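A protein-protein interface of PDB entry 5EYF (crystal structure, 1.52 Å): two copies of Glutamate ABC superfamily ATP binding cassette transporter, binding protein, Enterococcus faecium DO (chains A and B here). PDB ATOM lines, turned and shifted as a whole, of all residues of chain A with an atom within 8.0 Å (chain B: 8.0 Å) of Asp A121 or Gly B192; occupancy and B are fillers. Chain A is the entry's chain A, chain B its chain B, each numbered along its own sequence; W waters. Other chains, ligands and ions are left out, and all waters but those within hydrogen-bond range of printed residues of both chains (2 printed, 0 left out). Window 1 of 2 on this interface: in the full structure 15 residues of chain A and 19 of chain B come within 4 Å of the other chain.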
ATOM      1  N   LEU A 109      -5.875   4.786  36.423  1.00  0.00           N
ATOM      2  CA  LEU A 109      -4.526   4.508  35.948  1.00  0.00           C
ATOM      3  C   LEU A 109      -3.508   5.166  36.849  1.00  0.00           C
ATOM      4  O   LEU A 109      -3.687   6.315  37.271  1.00  0.00           O
ATOM      5  CB  LEU A 109      -4.298   5.056  34.548  1.00  0.00           C
ATOM      6  CG  LEU A 109      -5.296   4.627  33.492  1.00  0.00           C
ATOM      7  CD1 LEU A 109      -5.001   5.410  32.210  1.00  0.00           C
ATOM      8  CD2 LEU A 109      -5.173   3.141  33.279  1.00  0.00           C
ATOM      9  N   ILE A 117       0.843   9.798  29.396  1.00  0.00           N
ATOM     10  CA  ILE A 117      -0.488   9.229  29.528  1.00  0.00           C
ATOM     11  C   ILE A 117      -1.258  10.065  30.538  1.00  0.00           C
ATOM     12  O   ILE A 117      -0.854  10.178  31.698  1.00  0.00           O
ATOM     13  CB  ILE A 117      -0.407   7.755  29.950  1.00  0.00           C
ATOM     14  CG1 ILE A 117       0.279   6.952  28.836  1.00  0.00           C
ATOM     15  CG2 ILE A 117      -1.796   7.200  30.295  1.00  0.00           C
ATOM     16  CD1 ILE A 117       0.510   5.510  29.181  1.00  0.00           C
ATOM     17  N   LYS A 118      -2.349  10.681  30.091  1.00  0.00           N
ATOM     18  CA  LYS A 118      -3.199  11.455  30.978  1.00  0.00           C
ATOM     19  C   LYS A 118      -4.613  10.903  31.085  1.00  0.00           C
ATOM     20  O   LYS A 118      -5.397  11.427  31.881  1.00  0.00           O
ATOM     21  CB  LYS A 118      -3.244  12.924  30.534  1.00  0.00           C
ATOM     22  CG  LYS A 118      -1.939  13.684  30.800  1.00  0.00           C
ATOM     23  CD  LYS A 118      -1.990  15.127  30.305  1.00  0.00           C
ATOM     24  CE  LYS A 118      -2.219  16.122  31.445  1.00  0.00           C
ATOM     25  NZ  LYS A 118      -2.064  17.541  30.988  1.00  0.00           N
ATOM     26  N   SER A 119      -4.960   9.857  30.336  1.00  0.00           N
ATOM     27  CA  SER A 119      -6.311   9.312  30.386  1.00  0.00           C
ATOM     28  C   SER A 119      -6.315   7.915  29.785  1.00  0.00           C
ATOM     29  O   SER A 119      -5.394   7.531  29.063  1.00  0.00           O
ATOM     30  CB  SER A 119      -7.295  10.215  29.628  1.00  0.00           C
ATOM     31  OG  SER A 119      -7.842   9.524  28.531  1.00  0.00           O
ATOM     32  N   VAL A 120      -7.380   7.158  30.089  1.00  0.00           N
ATOM     33  CA  VAL A 120      -7.635   5.888  29.408  1.00  0.00           C
ATOM     34  C   VAL A 120      -7.660   6.057  27.887  1.00  0.00           C
ATOM     35  O   VAL A 120      -7.370   5.111  27.140  1.00  0.00           O
ATOM     36  CB  VAL A 120      -8.952   5.278  29.945  1.00  0.00           C
ATOM     37  CG1 VAL A 120     -10.140   6.150  29.544  1.00  0.00           C
ATOM     38  CG2 VAL A 120      -9.132   3.834  29.479  1.00  0.00           C
ATOM     39  N   ASP A 121      -7.992   7.257  27.396  1.00  0.00           N
ATOM     40  CA  ASP A 121      -7.966   7.492  25.956  1.00  0.00           C
ATOM     41  C   ASP A 121      -6.556   7.436  25.374  1.00  0.00           C
ATOM     42  O   ASP A 121      -6.409   7.223  24.167  1.00  0.00           O
ATOM     43  CB  ASP A 121      -8.584   8.847  25.619  1.00  0.00           C
ATOM     44  CG  ASP A 121      -9.949   9.049  26.242  1.00  0.00           C
ATOM     45  OD1 ASP A 121     -10.621   8.049  26.567  1.00  0.00           O
ATOM     46  OD2 ASP A 121     -10.356  10.221  26.400  1.00  0.00           O
ATOM     47  N   ASP A 122      -5.521   7.638  26.187  1.00  0.00           N
ATOM     48  CA  ASP A 122      -4.147   7.608  25.696  1.00  0.00           C
ATOM     49  C   ASP A 122      -3.574   6.194  25.594  1.00  0.00           C
ATOM     50  O   ASP A 122      -2.411   6.042  25.204  1.00  0.00           O
ATOM     51  CB  ASP A 122      -3.246   8.456  26.601  1.00  0.00           C
ATOM     52  CG  ASP A 122      -3.496   9.947  26.459  1.00  0.00           C
ATOM     53  OD1 ASP A 122      -3.805  10.393  25.339  1.00  0.00           O
ATOM     54  OD2 ASP A 122      -3.377  10.683  27.467  1.00  0.00           O
ATOM     55  N   LEU A 123      -4.350   5.166  25.933  1.00  0.00           N
ATOM     56  CA  LEU A 123      -3.876   3.780  25.972  1.00  0.00           C
ATOM     57  C   LEU A 123      -4.106   3.105  24.619  1.00  0.00           C
ATOM     58  O   LEU A 123      -4.968   2.242  24.449  1.00  0.00           O
ATOM     59  CB  LEU A 123      -4.573   3.012  27.085  1.00  0.00           C
ATOM     60  CG  LEU A 123      -4.239   3.454  28.504  1.00  0.00           C
ATOM     61  CD1 LEU A 123      -4.967   2.568  29.488  1.00  0.00           C
ATOM     62  CD2 LEU A 123      -2.753   3.377  28.711  1.00  0.00           C
ATOM     63  N   ASN A 124      -3.295   3.504  23.652  1.00  0.00           N
ATOM     64  CA  ASN A 124      -3.428   3.007  22.293  1.00  0.00           C
ATOM     65  C   ASN A 124      -2.519   1.793  22.082  1.00  0.00           C
ATOM     66  O   ASN A 124      -1.941   1.237  23.024  1.00  0.00           O
ATOM     67  CB  ASN A 124      -3.124   4.128  21.302  1.00  0.00           C
ATOM     68  CG  ASN A 124      -1.740   4.719  21.494  1.00  0.00           C
ATOM     69  OD1 ASN A 124      -0.781   4.006  21.784  1.00  0.00           O
ATOM     70  ND2 ASN A 124      -1.632   6.030  21.343  1.00  0.00           N
ATOM     71  N   ALA A 125      -2.353   1.395  20.820  1.00  0.00           N
ATOM     72  CA  ALA A 125      -1.582   0.199  20.512  1.00  0.00           C
ATOM     73  C   ALA A 125      -0.124   0.333  20.932  1.00  0.00           C
ATOM     74  O   ALA A 125       0.567  -0.680  21.054  1.00  0.00           O
ATOM     75  CB  ALA A 125      -1.672  -0.112  19.014  1.00  0.00           C
ATOM     76  N   THR A 127       0.898   1.297  23.852  1.00  0.00           N
ATOM     77  CA  THR A 127       1.030   1.244  25.302  1.00  0.00           C
ATOM     78  C   THR A 127       0.832  -0.170  25.842  1.00  0.00           C
ATOM     79  O   THR A 127       0.152  -1.005  25.241  1.00  0.00           O
ATOM     80  CB  THR A 127       0.043   2.204  25.972  1.00  0.00           C
ATOM     81  OG1 THR A 127      -1.299   1.804  25.678  1.00  0.00           O
ATOM     82  CG2 THR A 127       0.261   3.616  25.457  1.00  0.00           C
ATOM     83  N   HIS A 144     -12.184  -1.064  27.376  1.00  0.00           N
ATOM     84  CA  HIS A 144     -12.051   0.389  27.298  1.00  0.00           C
ATOM     85  C   HIS A 144     -10.853   0.825  26.471  1.00  0.00           C
ATOM     86  O   HIS A 144     -10.874   1.917  25.887  1.00  0.00           O
ATOM     87  CB  HIS A 144     -11.949   0.989  28.703  1.00  0.00           C
ATOM     88  CG  HIS A 144     -13.275   1.171  29.370  1.00  0.00           C
ATOM     89  ND1 HIS A 144     -13.915   0.154  30.045  1.00  0.00           N
ATOM     90  CD2 HIS A 144     -14.094   2.248  29.448  1.00  0.00           C
ATOM     91  CE1 HIS A 144     -15.065   0.597  30.520  1.00  0.00           C
ATOM     92  NE2 HIS A 144     -15.201   1.863  30.166  1.00  0.00           N
ATOM     93  N   ALA A 145      -9.810   0.005  26.416  1.00  0.00           N
ATOM     94  CA  ALA A 145      -8.602   0.289  25.644  1.00  0.00           C
ATOM     95  C   ALA A 145      -8.292  -0.943  24.807  1.00  0.00           C
ATOM     96  O   ALA A 145      -7.300  -1.642  25.047  1.00  0.00           O
ATOM     97  CB  ALA A 145      -7.436   0.655  26.564  1.00  0.00           C
ATOM     98  N   VAL A 191      -3.773   9.419  37.008  1.00  0.00           N
ATOM     99  CA  VAL A 191      -4.046  10.313  35.896  1.00  0.00           C
ATOM    100  C   VAL A 191      -5.395   9.956  35.303  1.00  0.00           C
ATOM    101  O   VAL A 191      -5.770   8.777  35.236  1.00  0.00           O
ATOM    102  CB  VAL A 191      -2.932  10.267  34.830  1.00  0.00           C
ATOM    103  CG1 VAL A 191      -1.593  10.847  35.400  1.00  0.00           C
ATOM    104  CG2 VAL A 191      -2.751   8.853  34.324  1.00  0.00           C
ATOM    105  N   GLY A 192      -6.149  10.992  34.941  1.00  0.00           N
ATOM    106  CA  GLY A 192      -7.327  10.825  34.115  1.00  0.00           C
ATOM    107  C   GLY A 192      -8.606  10.437  34.806  1.00  0.00           C
ATOM    108  O   GLY A 192      -9.484   9.861  34.156  1.00  0.00           O
ATOM    109  N   GLY A 193      -8.759  10.733  36.096  1.00  0.00           N
ATOM    110  CA  GLY A 193     -10.092  10.391  36.615  1.00  0.00           C
ATOM    111  C   GLY A 193     -10.360   8.892  36.619  1.00  0.00           C
ATOM    112  O   GLY A 193      -9.447   8.062  36.721  1.00  0.00           O
ATOM    113  N   THR A 194     -11.631   8.528  36.477  1.00  0.00           N
ATOM    114  CA  THR A 194     -12.018   7.119  36.498  1.00  0.00           C
ATOM    115  C   THR A 194     -12.814   6.776  35.253  1.00  0.00           C
ATOM    116  O   THR A 194     -13.475   7.641  34.679  1.00  0.00           O
ATOM    117  CB  THR A 194     -12.852   6.749  37.748  1.00  0.00           C
ATOM    118  OG1 THR A 194     -14.043   7.559  37.792  1.00  0.00           O
ATOM    119  CG2 THR A 194     -12.086   6.989  38.999  1.00  0.00           C
ATOM    120  N   PHE A 195     -12.789   5.498  34.849  1.00  0.00           N
ATOM    121  CA  PHE A 195     -13.539   5.101  33.659  1.00  0.00           C
ATOM    122  C   PHE A 195     -14.502   3.947  33.942  1.00  0.00           C
ATOM    123  O   PHE A 195     -15.126   3.409  33.004  1.00  0.00           O
ATOM    124  CB  PHE A 195     -12.608   4.780  32.460  1.00  0.00           C
ATOM    125  CG  PHE A 195     -11.527   3.753  32.746  1.00  0.00           C
ATOM    126  CD1 PHE A 195     -11.750   2.407  32.501  1.00  0.00           C
ATOM    127  CD2 PHE A 195     -10.288   4.146  33.239  1.00  0.00           C
ATOM    128  CE1 PHE A 195     -10.766   1.447  32.749  1.00  0.00           C
ATOM    129  CE2 PHE A 195      -9.295   3.203  33.482  1.00  0.00           C
ATOM    130  CZ  PHE A 195      -9.531   1.840  33.237  1.00  0.00           C
ATOM    131  N   GLN B 107     -19.110  13.548  36.835  1.00  0.00           N
ATOM    132  CA  GLN B 107     -18.872  14.701  35.970  1.00  0.00           C
ATOM    133  C   GLN B 107     -17.819  14.396  34.912  1.00  0.00           C
ATOM    134  O   GLN B 107     -16.844  13.694  35.169  1.00  0.00           O
ATOM    135  CB  GLN B 107     -18.464  15.913  36.799  1.00  0.00           C
ATOM    136  CG  GLN B 107     -18.503  17.208  35.982  1.00  0.00           C
ATOM    137  CD  GLN B 107     -18.435  18.430  36.861  1.00  0.00           C
ATOM    138  OE1 GLN B 107     -18.779  18.364  38.026  1.00  0.00           O
ATOM    139  NE2 GLN B 107     -17.953  19.541  36.317  1.00  0.00           N
ATOM    140  N   ALA B 108     -18.006  14.955  33.719  1.00  0.00           N
ATOM    141  CA  ALA B 108     -17.142  14.645  32.584  1.00  0.00           C
ATOM    142  C   ALA B 108     -17.017  15.862  31.685  1.00  0.00           C
ATOM    143  O   ALA B 108     -17.608  16.914  31.939  1.00  0.00           O
ATOM    144  CB  ALA B 108     -17.659  13.451  31.761  1.00  0.00           C
ATOM    145  N   LEU B 109     -16.222  15.700  30.629  1.00  0.00           N
ATOM    146  CA  LEU B 109     -15.931  16.752  29.660  1.00  0.00           C
ATOM    147  C   LEU B 109     -16.384  16.342  28.274  1.00  0.00           C
ATOM    148  O   LEU B 109     -16.142  15.217  27.845  1.00  0.00           O
ATOM    149  CB  LEU B 109     -14.444  17.036  29.549  1.00  0.00           C
ATOM    150  CG  LEU B 109     -13.713  17.549  30.779  1.00  0.00           C
ATOM    151  CD1 LEU B 109     -12.246  17.843  30.447  1.00  0.00           C
ATOM    152  CD2 LEU B 109     -14.392  18.780  31.370  1.00  0.00           C
ATOM    153  N   LEU B 110     -16.976  17.289  27.550  1.00  0.00           N
ATOM    154  CA  LEU B 110     -17.307  17.128  26.142  1.00  0.00           C
ATOM    155  C   LEU B 110     -16.491  18.138  25.342  1.00  0.00           C
ATOM    156  O   LEU B 110     -16.463  19.322  25.691  1.00  0.00           O
ATOM    157  CB  LEU B 110     -18.811  17.370  25.925  1.00  0.00           C
ATOM    158  CG  LEU B 110     -19.391  17.181  24.518  1.00  0.00           C
ATOM    159  CD1 LEU B 110     -19.667  15.714  24.307  1.00  0.00           C
ATOM    160  CD2 LEU B 110     -20.670  18.009  24.298  1.00  0.00           C
ATOM    161  N   VAL B 111     -15.807  17.665  24.295  1.00  0.00           N
ATOM    162  CA  VAL B 111     -14.980  18.504  23.433  1.00  0.00           C
ATOM    163  C   VAL B 111     -15.260  18.136  21.982  1.00  0.00           C
ATOM    164  O   VAL B 111     -15.811  17.075  21.684  1.00  0.00           O
ATOM    165  CB  VAL B 111     -13.462  18.340  23.749  1.00  0.00           C
ATOM    166  CG1 VAL B 111     -13.155  18.742  25.190  1.00  0.00           C
ATOM    167  CG2 VAL B 111     -13.014  16.911  23.509  1.00  0.00           C
ATOM    168  N   ILE B 117      -7.480  18.799  24.431  1.00  0.00           N
ATOM    169  CA  ILE B 117      -7.963  18.512  25.784  1.00  0.00           C
ATOM    170  C   ILE B 117      -8.418  17.055  25.849  1.00  0.00           C
ATOM    171  O   ILE B 117      -9.341  16.655  25.134  1.00  0.00           O
ATOM    172  CB  ILE B 117      -9.105  19.475  26.159  1.00  0.00           C
ATOM    173  CG1 ILE B 117      -8.554  20.906  26.270  1.00  0.00           C
ATOM    174  CG2 ILE B 117      -9.824  19.046  27.446  1.00  0.00           C
ATOM    175  CD1 ILE B 117      -9.622  21.974  26.366  1.00  0.00           C
ATOM    176  N   LYS B 118      -7.777  16.257  26.716  1.00  0.00           N
ATOM    177  CA  LYS B 118      -8.079  14.834  26.834  1.00  0.00           C
ATOM    178  C   LYS B 118      -8.670  14.443  28.176  1.00  0.00           C
ATOM    179  O   LYS B 118      -9.125  13.299  28.329  1.00  0.00           O
ATOM    180  CB  LYS B 118      -6.818  13.986  26.632  1.00  0.00           C
ATOM    181  CG  LYS B 118      -5.947  14.370  25.459  1.00  0.00           C
ATOM    182  CD  LYS B 118      -4.552  13.846  25.756  1.00  0.00           C
ATOM    183  CE  LYS B 118      -3.643  13.877  24.540  1.00  0.00           C
ATOM    184  NZ  LYS B 118      -2.446  13.002  24.759  1.00  0.00           N
ATOM    185  N   SER B 119      -8.641  15.335  29.151  1.00  0.00           N
ATOM    186  CA  SER B 119      -9.152  15.042  30.476  1.00  0.00           C
ATOM    187  C   SER B 119      -9.161  16.338  31.262  1.00  0.00           C
ATOM    188  O   SER B 119      -8.671  17.379  30.805  1.00  0.00           O
ATOM    189  CB  SER B 119      -8.298  14.002  31.198  1.00  0.00           C
ATOM    190  OG  SER B 119      -7.151  14.616  31.766  1.00  0.00           O
ATOM    191  N   VAL B 120      -9.710  16.245  32.473  1.00  0.00           N
ATOM    192  CA  VAL B 120      -9.751  17.392  33.357  1.00  0.00           C
ATOM    193  C   VAL B 120      -8.345  17.906  33.638  1.00  0.00           C
ATOM    194  O   VAL B 120      -8.171  19.089  33.915  1.00  0.00           O
ATOM    195  CB  VAL B 120     -10.518  17.001  34.638  1.00  0.00           C
ATOM    196  CG1 VAL B 120      -9.688  16.045  35.482  1.00  0.00           C
ATOM    197  CG2 VAL B 120     -10.980  18.242  35.409  1.00  0.00           C
ATOM    198  N   ASP B 121      -7.327  17.052  33.518  1.00  0.00           N
ATOM    199  CA  ASP B 121      -5.964  17.481  33.799  1.00  0.00           C
ATOM    200  C   ASP B 121      -5.455  18.496  32.775  1.00  0.00           C
ATOM    201  O   ASP B 121      -4.484  19.207  33.045  1.00  0.00           O
ATOM    202  CB  ASP B 121      -5.021  16.263  33.852  1.00  0.00           C
ATOM    203  CG  ASP B 121      -5.282  15.350  35.060  1.00  0.00           C
ATOM    204  OD1 ASP B 121      -5.912  15.819  36.029  1.00  0.00           O
ATOM    205  OD2 ASP B 121      -4.826  14.168  35.056  1.00  0.00           O
ATOM    206  N   GLU B 189     -17.249  14.522  21.434  1.00  0.00           N
ATOM    207  CA  GLU B 189     -17.114  13.277  22.181  1.00  0.00           C
ATOM    208  C   GLU B 189     -16.789  13.581  23.635  1.00  0.00           C
ATOM    209  O   GLU B 189     -16.220  14.634  23.970  1.00  0.00           O
ATOM    210  CB  GLU B 189     -16.034  12.357  21.572  1.00  0.00           C
ATOM    211  CG  GLU B 189     -14.609  12.897  21.623  1.00  0.00           C
ATOM    212  CD  GLU B 189     -13.611  11.998  20.893  1.00  0.00           C
ATOM    213  OE1 GLU B 189     -13.996  10.874  20.523  1.00  0.00           O
ATOM    214  OE2 GLU B 189     -12.448  12.413  20.677  1.00  0.00           O
ATOM    215  N   LEU B 190     -17.134  12.628  24.500  1.00  0.00           N
ATOM    216  CA  LEU B 190     -16.657  12.661  25.882  1.00  0.00           C
ATOM    217  C   LEU B 190     -15.191  12.252  25.922  1.00  0.00           C
ATOM    218  O   LEU B 190     -14.755  11.376  25.164  1.00  0.00           O
ATOM    219  CB  LEU B 190     -17.486  11.729  26.794  1.00  0.00           C
ATOM    220  CG  LEU B 190     -18.866  12.182  27.293  1.00  0.00           C
ATOM    221  CD1 LEU B 190     -19.859  12.202  26.127  1.00  0.00           C
ATOM    222  CD2 LEU B 190     -19.385  11.275  28.388  1.00  0.00           C
ATOM    223  N   VAL B 191     -14.412  12.923  26.766  1.00  0.00           N
ATOM    224  CA  VAL B 191     -12.992  12.612  26.902  1.00  0.00           C
ATOM    225  C   VAL B 191     -12.641  12.585  28.374  1.00  0.00           C
ATOM    226  O   VAL B 191     -13.128  13.410  29.163  1.00  0.00           O
ATOM    227  CB  VAL B 191     -12.068  13.621  26.167  1.00  0.00           C
ATOM    228  CG1 VAL B 191     -12.318  13.605  24.667  1.00  0.00           C
ATOM    229  CG2 VAL B 191     -12.223  15.043  26.711  1.00  0.00           C
ATOM    230  N   GLY B 192     -11.768  11.647  28.733  1.00  0.00           N
ATOM    231  CA  GLY B 192     -11.177  11.598  30.053  1.00  0.00           C
ATOM    232  C   GLY B 192     -11.996  10.919  31.125  1.00  0.00           C
ATOM    233  O   GLY B 192     -11.674  11.079  32.310  1.00  0.00           O
ATOM    234  N   GLY B 193     -13.043  10.173  30.772  1.00  0.00           N
ATOM    235  CA  GLY B 193     -13.733   9.484  31.872  1.00  0.00           C
ATOM    236  C   GLY B 193     -14.493  10.454  32.770  1.00  0.00           C
ATOM    237  O   GLY B 193     -15.002  11.490  32.310  1.00  0.00           O
ATOM    238  N   THR B 194     -14.565  10.131  34.071  1.00  0.00           N
ATOM    239  CA  THR B 194     -15.259  11.003  35.018  1.00  0.00           C
ATOM    240  C   THR B 194     -14.296  11.449  36.102  1.00  0.00           C
ATOM    241  O   THR B 194     -13.365  10.721  36.459  1.00  0.00           O
ATOM    242  CB  THR B 194     -16.504  10.323  35.674  1.00  0.00           C
ATOM    243  OG1 THR B 194     -16.121   9.132  36.360  1.00  0.00           O
ATOM    244  CG2 THR B 194     -17.589  10.008  34.628  1.00  0.00           C
ATOM    245  N   PHE B 195     -14.518  12.643  36.647  1.00  0.00           N
ATOM    246  CA  PHE B 195     -13.646  13.126  37.710  1.00  0.00           C
ATOM    247  C   PHE B 195     -14.414  13.468  38.983  1.00  0.00           C
ATOM    248  O   PHE B 195     -13.820  13.990  39.937  1.00  0.00           O
ATOM    249  CB  PHE B 195     -12.781  14.319  37.236  1.00  0.00           C
ATOM    250  CG  PHE B 195     -13.556  15.479  36.650  1.00  0.00           C
ATOM    251  CD1 PHE B 195     -13.984  16.528  37.457  1.00  0.00           C
ATOM    252  CD2 PHE B 195     -13.852  15.515  35.293  1.00  0.00           C
ATOM    253  CE1 PHE B 195     -14.711  17.615  36.896  1.00  0.00           C
ATOM    254  CE2 PHE B 195     -14.559  16.581  34.730  1.00  0.00           C
ATOM    255  CZ  PHE B 195     -14.996  17.620  35.525  1.00  0.00           C
HETATM  256  O   HOH W   1     -13.855   9.990  39.412  1.00  0.00           O
HETATM  257  O   HOH W   2     -16.372   6.606  34.971  1.00  0.00           O
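Of the 18 printed residues of chain A, 7 touch a printed residue of chain B.
Of the 17 printed residues of chain B, 7 touch a printed residue of chain A.
Among the printed residues, Asp or Glu carboxylates within 4 Å of a Lys or Arg side-chain nitrogen of the other chain: Asp A122 with Lys B118 (3.0 Å).
Lys A118 touches Ser B119, and with the chains exchanged Ser A119 touches Lys B118.
Asp A121 touches Gly B192, and with the chains exchanged Gly A192 touches Asp B121.
Gly B192 touches its own counterpart, Gly A192.
Thr B194 touches its own counterpart, Thr A194.
Positions printed for both chains: 109, 117, 118, 119, 120, 121, 191, 192, 193, 194 and 195.
Water W2 lies within hydrogen-bond range of the side-chain hydroxyl (OG1) of Thr B194 (2.9 Å) and the backbone carbonyl oxygen (O) of Thr A194 (3.1 Å).
Water W1 lies within hydrogen-bond range of the side-chain hydroxyl (OG1) of Thr A194 and the backbone carbonyl oxygen (O) of Thr B194.
Of the printed residues of chain B, Lys A118 touches Ser B119 (3.6 Å) and Asp B121 (3.6 Å).
Asp A121 touches just these residues of chain B: Lys B118, Val B191 and Gly B192.
Printed residues of chain B within 4 Å of Thr A194: Gly B193 and Thr B194.
Of the printed residues of chain A, Val B191 touches Asp A121.
Gly B192 touches just these residues of chain A: Asp A121 and Gly A192.
Of the printed residues of chain A, Thr B194 touches Gly A193 and Thr A194.
The nearest residue of chain A that does not touch Gly B192 is Ser A119 (4.1 Å).
The nearest printed residue of chain B that does not touch Ser A119 is Gly B192 (4.1 Å).
The backbone carbonyl oxygen (O) of Thr A194 sits at hydrogen-bond distance from the backbone NH (N) of Thr B194 (2.8 Å).
O of Gly A192 lies close to O of Gly B192 (3.1 Å).
The backbone NH (N) of Gly A192 is in hydrogen-bond range of the side-chain carboxylate (OD2) of Asp B121, 3.4 Å away.
OD1 of Asp A122 is in salt-bridge range of NZ of Lys B118.
OD2 of Asp A121 sits at hydrogen-bond distance from N of Gly B192, 3.1 Å away.
Among the printed residues, pairs that only touch across the chains: Lys A118 with Ser B119, Lys A118 with Asp B121, Ser A119 with Lys B118, Asp A121 with Lys B118, Asp A121 with Val B191, Gly A193 with Thr B194 and Thr A194 with Gly B193.
The side-chain hydroxyl (OG) of Ser B119 lies close to the backbone NH (N) of Asp B121 (3.0 Å).
N of Val B191 sits at hydrogen-bond distance from O of Leu B109, 3.1 Å away.
The backbone NH (N) of Ser A119 is in hydrogen-bond range of the side-chain carboxylate (OD2) of Asp A122.
The side-chain hydroxyl (OG) of Ser A119 sits at hydrogen-bond distance from the backbone NH (N) of Asp A121 (2.5 Å).
The side-chain carboxylate (OD2) of Asp A122 sits at hydrogen-bond distance from the backbone NH (N) of Lys A118 (2.8 Å).
O of Lys A118 sits close to N of Gly A192 (3.2 Å).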
